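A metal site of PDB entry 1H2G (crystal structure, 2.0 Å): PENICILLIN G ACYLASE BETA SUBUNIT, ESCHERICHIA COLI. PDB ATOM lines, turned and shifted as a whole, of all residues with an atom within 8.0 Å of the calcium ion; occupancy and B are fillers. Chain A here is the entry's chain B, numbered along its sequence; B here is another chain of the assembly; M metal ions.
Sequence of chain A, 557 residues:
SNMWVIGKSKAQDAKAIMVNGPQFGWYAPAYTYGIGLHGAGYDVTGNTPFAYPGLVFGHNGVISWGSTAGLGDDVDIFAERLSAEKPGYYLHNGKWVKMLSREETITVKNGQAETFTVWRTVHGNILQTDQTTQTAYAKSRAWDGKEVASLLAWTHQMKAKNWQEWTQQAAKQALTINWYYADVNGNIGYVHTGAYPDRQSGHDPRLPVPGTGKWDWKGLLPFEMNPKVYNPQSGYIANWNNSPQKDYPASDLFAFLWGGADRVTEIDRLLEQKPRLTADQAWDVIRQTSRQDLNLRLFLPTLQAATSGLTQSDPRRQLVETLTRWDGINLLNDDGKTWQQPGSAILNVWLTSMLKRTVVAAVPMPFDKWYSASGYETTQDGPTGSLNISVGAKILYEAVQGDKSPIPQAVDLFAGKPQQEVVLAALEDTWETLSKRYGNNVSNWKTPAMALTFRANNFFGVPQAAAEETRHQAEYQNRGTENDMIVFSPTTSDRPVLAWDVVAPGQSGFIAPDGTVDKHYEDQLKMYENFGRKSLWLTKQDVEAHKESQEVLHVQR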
ATOM      1  N   GLY A  72       3.606 -28.240  14.462  1.00  0.00           N
ATOM      2  CA  GLY A  72       3.376 -26.960  13.801  1.00  0.00           C
ATOM      3  C   GLY A  72       4.463 -26.771  12.743  1.00  0.00           C
ATOM      4  O   GLY A  72       5.367 -27.615  12.626  1.00  0.00           O
ATOM      5  N   ASP A  73       4.380 -25.690  11.969  1.00  0.00           N
ATOM      6  CA  ASP A  73       5.387 -25.435  10.947  1.00  0.00           C
ATOM      7  C   ASP A  73       6.384 -24.389  11.437  1.00  0.00           C
ATOM      8  O   ASP A  73       6.150 -23.186  11.317  1.00  0.00           O
ATOM      9  CB  ASP A  73       4.734 -24.965   9.643  1.00  0.00           C
ATOM     10  CG  ASP A  73       5.724 -24.811   8.507  1.00  0.00           C
ATOM     11  OD1 ASP A  73       6.958 -24.750   8.764  1.00  0.00           O
ATOM     12  OD2 ASP A  73       5.343 -24.711   7.318  1.00  0.00           O
ATOM     13  N   ASP A  74       7.517 -24.864  11.961  1.00  0.00           N
ATOM     14  CA  ASP A  74       8.569 -23.990  12.467  1.00  0.00           C
ATOM     15  C   ASP A  74       9.887 -24.170  11.709  1.00  0.00           C
ATOM     16  O   ASP A  74      10.976 -23.793  12.197  1.00  0.00           O
ATOM     17  CB  ASP A  74       8.773 -24.204  13.989  1.00  0.00           C
ATOM     18  CG  ASP A  74       9.221 -25.627  14.358  1.00  0.00           C
ATOM     19  OD1 ASP A  74       9.355 -26.512  13.482  1.00  0.00           O
ATOM     20  OD2 ASP A  74       9.439 -25.968  15.542  1.00  0.00           O
ATOM     21  N   VAL A  75       9.801 -24.778  10.526  1.00  0.00           N
ATOM     22  CA  VAL A  75      10.964 -25.017   9.691  1.00  0.00           C
ATOM     23  C   VAL A  75      10.669 -24.692   8.228  1.00  0.00           C
ATOM     24  O   VAL A  75       9.718 -25.233   7.647  1.00  0.00           O
ATOM     25  CB  VAL A  75      11.408 -26.491   9.743  1.00  0.00           C
ATOM     26  CG1 VAL A  75      12.536 -26.732   8.770  1.00  0.00           C
ATOM     27  CG2 VAL A  75      11.793 -26.920  11.160  1.00  0.00           C
ATOM     28  N   ASP A  76      11.472 -23.806   7.630  1.00  0.00           N
ATOM     29  CA  ASP A  76      11.316 -23.442   6.226  1.00  0.00           C
ATOM     30  C   ASP A  76      12.700 -23.660   5.586  1.00  0.00           C
ATOM     31  O   ASP A  76      13.729 -23.528   6.250  1.00  0.00           O
ATOM     32  CB  ASP A  76      10.947 -21.988   6.005  1.00  0.00           C
ATOM     33  CG  ASP A  76       9.573 -21.638   6.487  1.00  0.00           C
ATOM     34  OD1 ASP A  76       8.706 -22.561   6.622  1.00  0.00           O
ATOM     35  OD2 ASP A  76       9.278 -20.431   6.719  1.00  0.00           O
ATOM     36  N   ILE A  77      12.695 -23.961   4.288  1.00  0.00           N
ATOM     37  CA  ILE A  77      13.899 -24.190   3.531  1.00  0.00           C
ATOM     38  C   ILE A  77      14.214 -23.015   2.617  1.00  0.00           C
ATOM     39  O   ILE A  77      13.349 -22.571   1.869  1.00  0.00           O
ATOM     40  CB  ILE A  77      13.700 -25.448   2.665  1.00  0.00           C
ATOM     41  CG1 ILE A  77      13.394 -26.645   3.552  1.00  0.00           C
ATOM     42  CG2 ILE A  77      14.931 -25.731   1.779  1.00  0.00           C
ATOM     43  CD1 ILE A  77      14.446 -26.927   4.608  1.00  0.00           C
ATOM     44  N   SER A 140      16.124 -23.668   7.904  1.00  0.00           N
ATOM     45  CA  SER A 140      15.926 -22.658   8.928  1.00  0.00           C
ATOM     46  C   SER A 140      14.854 -23.089   9.948  1.00  0.00           C
ATOM     47  O   SER A 140      13.685 -23.315   9.615  1.00  0.00           O
ATOM     48  CB  SER A 140      15.606 -21.328   8.236  1.00  0.00           C
ATOM     49  OG  SER A 140      15.361 -20.276   9.145  1.00  0.00           O
ATOM     50  N   PRO A 197       7.965 -18.468  12.908  1.00  0.00           N
ATOM     51  CA  PRO A 197       8.439 -17.278  12.194  1.00  0.00           C
ATOM     52  C   PRO A 197       7.351 -16.369  11.726  1.00  0.00           C
ATOM     53  O   PRO A 197       6.252 -16.839  11.409  1.00  0.00           O
ATOM     54  CB  PRO A 197       9.065 -17.845  10.913  1.00  0.00           C
ATOM     55  CG  PRO A 197       8.571 -19.259  10.768  1.00  0.00           C
ATOM     56  CD  PRO A 197       7.916 -19.662  12.057  1.00  0.00           C
ATOM     57  N   ARG A 199       6.528 -14.559   8.833  1.00  0.00           N
ATOM     58  CA  ARG A 199       6.909 -14.543   7.428  1.00  0.00           C
ATOM     59  C   ARG A 199       6.456 -13.372   6.578  1.00  0.00           C
ATOM     60  O   ARG A 199       5.437 -12.750   6.854  1.00  0.00           O
ATOM     61  CB  ARG A 199       6.371 -15.832   6.796  1.00  0.00           C
ATOM     62  CG  ARG A 199       6.752 -17.126   7.523  1.00  0.00           C
ATOM     63  CD  ARG A 199       6.200 -18.355   6.814  1.00  0.00           C
ATOM     64  NE  ARG A 199       6.737 -19.623   7.285  1.00  0.00           N
ATOM     65  CZ  ARG A 199       6.194 -20.372   8.228  1.00  0.00           C
ATOM     66  NH1 ARG A 199       5.108 -19.968   8.886  1.00  0.00           N
ATOM     67  NH2 ARG A 199       6.754 -21.516   8.539  1.00  0.00           N
ATOM     68  N   HIS A 203       4.397 -15.614   1.442  1.00  0.00           N
ATOM     69  CA  HIS A 203       5.251 -16.752   1.686  1.00  0.00           C
ATOM     70  C   HIS A 203       4.426 -18.025   1.930  1.00  0.00           C
ATOM     71  O   HIS A 203       3.753 -18.153   2.944  1.00  0.00           O
ATOM     72  CB  HIS A 203       6.202 -16.430   2.860  1.00  0.00           C
ATOM     73  CG  HIS A 203       7.159 -17.531   3.213  1.00  0.00           C
ATOM     74  ND1 HIS A 203       8.292 -17.299   3.953  1.00  0.00           N
ATOM     75  CD2 HIS A 203       7.144 -18.859   2.950  1.00  0.00           C
ATOM     76  CE1 HIS A 203       8.940 -18.448   4.130  1.00  0.00           C
ATOM     77  NE2 HIS A 203       8.266 -19.405   3.526  1.00  0.00           N
ATOM     78  N   ASP A 204       4.465 -18.954   0.973  1.00  0.00           N
ATOM     79  CA  ASP A 204       3.762 -20.246   1.083  1.00  0.00           C
ATOM     80  C   ASP A 204       4.714 -21.140   1.914  1.00  0.00           C
ATOM     81  O   ASP A 204       5.731 -21.636   1.414  1.00  0.00           O
ATOM     82  CB  ASP A 204       3.520 -20.837  -0.300  1.00  0.00           C
ATOM     83  CG  ASP A 204       2.637 -22.069  -0.255  1.00  0.00           C
ATOM     84  OD1 ASP A 204       2.679 -22.802   0.764  1.00  0.00           O
ATOM     85  OD2 ASP A 204       1.837 -22.356  -1.192  1.00  0.00           O
ATOM     86  N   PRO A 205       4.347 -21.430   3.166  1.00  0.00           N
ATOM     87  CA  PRO A 205       5.216 -22.214   4.066  1.00  0.00           C
ATOM     88  C   PRO A 205       5.399 -23.690   3.781  1.00  0.00           C
ATOM     89  O   PRO A 205       6.161 -24.352   4.492  1.00  0.00           O
ATOM     90  CB  PRO A 205       4.565 -22.010   5.438  1.00  0.00           C
ATOM     91  CG  PRO A 205       3.106 -21.721   5.146  1.00  0.00           C
ATOM     92  CD  PRO A 205       3.037 -21.111   3.777  1.00  0.00           C
ATOM     93  N   ARG A 206       4.728 -24.203   2.774  1.00  0.00           N
ATOM     94  CA  ARG A 206       4.846 -25.617   2.400  1.00  0.00           C
ATOM     95  C   ARG A 206       5.917 -25.841   1.356  1.00  0.00           C
ATOM     96  O   ARG A 206       6.238 -26.992   1.058  1.00  0.00           O
ATOM     97  CB  ARG A 206       3.529 -26.049   1.759  1.00  0.00           C
ATOM     98  CG  ARG A 206       2.276 -25.783   2.608  1.00  0.00           C
ATOM     99  CD  ARG A 206       0.967 -26.003   1.862  1.00  0.00           C
ATOM    100  NE  ARG A 206       0.808 -25.095   0.722  1.00  0.00           N
ATOM    101  CZ  ARG A 206      -0.175 -25.132  -0.163  1.00  0.00           C
ATOM    102  NH1 ARG A 206      -1.140 -26.055  -0.073  1.00  0.00           N
ATOM    103  NH2 ARG A 206      -0.214 -24.236  -1.155  1.00  0.00           N
ATOM    104  N   LEU A 207       6.485 -24.754   0.825  1.00  0.00           N
ATOM    105  CA  LEU A 207       7.498 -24.797  -0.231  1.00  0.00           C
ATOM    106  C   LEU A 207       8.706 -23.906   0.047  1.00  0.00           C
ATOM    107  O   LEU A 207       8.581 -22.931   0.763  1.00  0.00           O
ATOM    108  CB  LEU A 207       6.796 -24.304  -1.510  1.00  0.00           C
ATOM    109  CG  LEU A 207       5.570 -25.147  -1.901  1.00  0.00           C
ATOM    110  CD1 LEU A 207       4.659 -24.414  -2.880  1.00  0.00           C
ATOM    111  CD2 LEU A 207       6.011 -26.460  -2.501  1.00  0.00           C
ATOM    112  N   PRO A 208       9.874 -24.210  -0.514  1.00  0.00           N
ATOM    113  CA  PRO A 208      11.051 -23.370  -0.231  1.00  0.00           C
ATOM    114  C   PRO A 208      10.936 -21.950  -0.720  1.00  0.00           C
ATOM    115  O   PRO A 208      10.088 -21.673  -1.579  1.00  0.00           O
ATOM    116  CB  PRO A 208      12.185 -24.087  -0.988  1.00  0.00           C
ATOM    117  CG  PRO A 208      11.719 -25.456  -1.191  1.00  0.00           C
ATOM    118  CD  PRO A 208      10.212 -25.313  -1.423  1.00  0.00           C
ATOM    119  N   TRP A 217      12.708 -14.150   6.990  1.00  0.00           N
ATOM    120  CA  TRP A 217      11.671 -13.969   7.992  1.00  0.00           C
ATOM    121  C   TRP A 217      11.806 -12.578   8.633  1.00  0.00           C
ATOM    122  O   TRP A 217      12.906 -12.088   8.800  1.00  0.00           O
ATOM    123  CB  TRP A 217      11.864 -14.981   9.114  1.00  0.00           C
ATOM    124  CG  TRP A 217      11.602 -16.410   8.768  1.00  0.00           C
ATOM    125  CD1 TRP A 217      10.887 -16.890   7.717  1.00  0.00           C
ATOM    126  CD2 TRP A 217      12.055 -17.557   9.489  1.00  0.00           C
ATOM    127  NE1 TRP A 217      10.858 -18.262   7.753  1.00  0.00           N
ATOM    128  CE2 TRP A 217      11.571 -18.697   8.830  1.00  0.00           C
ATOM    129  CE3 TRP A 217      12.816 -17.737  10.653  1.00  0.00           C
ATOM    130  CZ2 TRP A 217      11.807 -19.994   9.289  1.00  0.00           C
ATOM    131  CZ3 TRP A 217      13.062 -19.029  11.103  1.00  0.00           C
ATOM    132  CH2 TRP A 217      12.564 -20.132  10.413  1.00  0.00           C
ATOM    133  N   ALA A 250      -0.559 -26.798  10.063  1.00  0.00           N
ATOM    134  CA  ALA A 250       0.351 -27.854  10.479  1.00  0.00           C
ATOM    135  C   ALA A 250       1.699 -27.754   9.742  1.00  0.00           C
ATOM    136  O   ALA A 250       1.884 -26.945   8.840  1.00  0.00           O
ATOM    137  CB  ALA A 250      -0.263 -29.175  10.126  1.00  0.00           C
ATOM    138  N   SER A 251       2.597 -28.627  10.179  1.00  0.00           N
ATOM    139  CA  SER A 251       3.921 -28.794   9.613  1.00  0.00           C
ATOM    140  C   SER A 251       3.781 -28.989   8.121  1.00  0.00           C
ATOM    141  O   SER A 251       2.767 -29.539   7.670  1.00  0.00           O
ATOM    142  CB  SER A 251       4.467 -30.132  10.148  1.00  0.00           C
ATOM    143  OG  SER A 251       5.594 -30.590   9.414  1.00  0.00           O
ATOM    144  N   ASP A 252       4.784 -28.564   7.367  1.00  0.00           N
ATOM    145  CA  ASP A 252       4.769 -28.737   5.908  1.00  0.00           C
ATOM    146  C   ASP A 252       5.036 -30.197   5.486  1.00  0.00           C
ATOM    147  O   ASP A 252       4.867 -30.521   4.320  1.00  0.00           O
ATOM    148  CB  ASP A 252       5.720 -27.804   5.196  1.00  0.00           C
ATOM    149  CG  ASP A 252       7.166 -27.964   5.628  1.00  0.00           C
ATOM    150  OD1 ASP A 252       7.721 -29.069   5.449  1.00  0.00           O
ATOM    151  OD2 ASP A 252       7.812 -27.018   6.134  1.00  0.00           O
ATOM    152  N   LEU A 253       5.416 -31.071   6.429  1.00  0.00           N
ATOM    153  CA  LEU A 253       5.683 -32.480   6.095  1.00  0.00           C
ATOM    154  C   LEU A 253       4.460 -33.051   5.345  1.00  0.00           C
ATOM    155  O   LEU A 253       3.344 -33.008   5.854  1.00  0.00           O
ATOM    156  CB  LEU A 253       6.023 -33.292   7.356  1.00  0.00           C
ATOM    157  CG  LEU A 253       6.388 -34.761   7.092  1.00  0.00           C
ATOM    158  CD1 LEU A 253       7.717 -34.818   6.361  1.00  0.00           C
ATOM    159  CD2 LEU A 253       6.476 -35.591   8.346  1.00  0.00           C
ATOM    160  N   SER B 149      10.603 -31.342  11.585  1.00  0.00           N
ATOM    161  CA  SER B 149       9.925 -32.008  10.471  1.00  0.00           C
ATOM    162  C   SER B 149       9.587 -31.149   9.275  1.00  0.00           C
ATOM    163  O   SER B 149       8.842 -30.179   9.385  1.00  0.00           O
ATOM    164  CB  SER B 149       8.591 -32.620  10.955  1.00  0.00           C
ATOM    165  OG  SER B 149       8.797 -33.677  11.867  1.00  0.00           O
ATOM    166  N   THR B 150      10.116 -31.516   8.110  1.00  0.00           N
ATOM    167  CA  THR B 150       9.835 -30.767   6.896  1.00  0.00           C
ATOM    168  C   THR B 150      10.113 -31.598   5.646  1.00  0.00           C
ATOM    169  O   THR B 150      10.948 -32.493   5.689  1.00  0.00           O
ATOM    170  CB  THR B 150      10.669 -29.493   6.851  1.00  0.00           C
ATOM    171  OG1 THR B 150      10.457 -28.815   5.609  1.00  0.00           O
ATOM    172  CG2 THR B 150      12.177 -29.825   6.882  1.00  0.00           C
ATOM    173  N   SER B 151       9.354 -31.337   4.579  1.00  0.00           N
ATOM    174  CA  SER B 151       9.530 -32.014   3.296  1.00  0.00           C
ATOM    175  C   SER B 151       9.367 -30.989   2.157  1.00  0.00           C
ATOM    176  O   SER B 151       9.027 -31.359   1.042  1.00  0.00           O
ATOM    177  CB  SER B 151       8.532 -33.169   3.118  1.00  0.00           C
ATOM    178  OG  SER B 151       7.184 -32.724   3.013  1.00  0.00           O
ATOM    179  N   GLU B 152       9.658 -29.706   2.441  1.00  0.00           N
ATOM    180  CA  GLU B 152       9.514 -28.648   1.428  1.00  0.00           C
ATOM    181  C   GLU B 152      10.159 -28.919   0.058  1.00  0.00           C
ATOM    182  O   GLU B 152       9.559 -28.652  -0.969  1.00  0.00           O
ATOM    183  CB  GLU B 152       9.964 -27.277   1.955  1.00  0.00           C
ATOM    184  CG  GLU B 152       9.141 -26.675   3.090  1.00  0.00           C
ATOM    185  CD  GLU B 152       9.638 -25.305   3.472  1.00  0.00           C
ATOM    186  OE1 GLU B 152      10.570 -24.775   2.776  1.00  0.00           O
ATOM    187  OE2 GLU B 152       9.125 -24.725   4.460  1.00  0.00           O
ATOM    188  N   ASN B 155       8.091 -31.507  -1.509  1.00  0.00           N
ATOM    189  CA  ASN B 155       6.770 -30.911  -1.788  1.00  0.00           C
ATOM    190  C   ASN B 155       6.852 -30.154  -3.128  1.00  0.00           C
ATOM    191  O   ASN B 155       5.944 -30.226  -3.976  1.00  0.00           O
ATOM    192  CB  ASN B 155       6.330 -29.960  -0.688  1.00  0.00           C
ATOM    193  CG  ASN B 155       6.049 -30.645   0.641  1.00  0.00           C
ATOM    194  OD1 ASN B 155       5.962 -31.877   0.737  1.00  0.00           O
ATOM    195  ND2 ASN B 155       5.913 -29.841   1.692  1.00  0.00           N
HETATM  196 CA    CA M   1       7.721 -24.703   6.283  1.00  0.00          CA
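Six residues have an atom within 4 Å of the calcium ion: Asp 73, Val 75, Asp 76, Pro 205, Asp 252 and Glu 152 of chain B.
The calcium ion is bound by OE2 of Glu 152 of chain B (2.3 Å), OD2 of Asp 252 (2.3 Å), OD1 of Asp 76 (2.4 Å), O of Pro 205 (2.4 Å), O of Val 75 (2.5 Å), OD2 of Asp 73 (2.6 Å) and OD1 of Asp 73 (2.6 Å).
N of Ser 140 lies within hydrogen-bond range of O of Asp 76 (2.9 Å).
The backbone NH (N) of Glu 152 of chain B is in hydrogen-bond range of the side-chain hydroxyl (OG1) of Thr 150 of chain B (3.4 Å).
The side-chain carboxylate of Asp 76 lies within hydrogen-bond range of the indole nitrogen of Trp 217 (2.9 Å).
The side-chain carboxylate (OD2) of Asp 76 lies within salt-bridge range of the guanidinium group (NE) of Arg 199 (2.7 Å).
OD1 of Asp 252 sits at hydrogen-bond distance from N of Ser 151 of chain B (2.9 Å).
The backbone carbonyl oxygen of Asp 252 lies within hydrogen-bond range of the side-chain amide nitrogen of Asn 155 of chain B (2.9 Å).
The backbone NH (N) of Ile 77 is in hydrogen-bond range of the side-chain carboxylate (OE1) of Glu 152 of chain B (2.7 Å).
The backbone carbonyl oxygen (O) of Asp 73 is in hydrogen-bond range of the guanidinium group (NH2) of Arg 199, 3.3 Å away.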
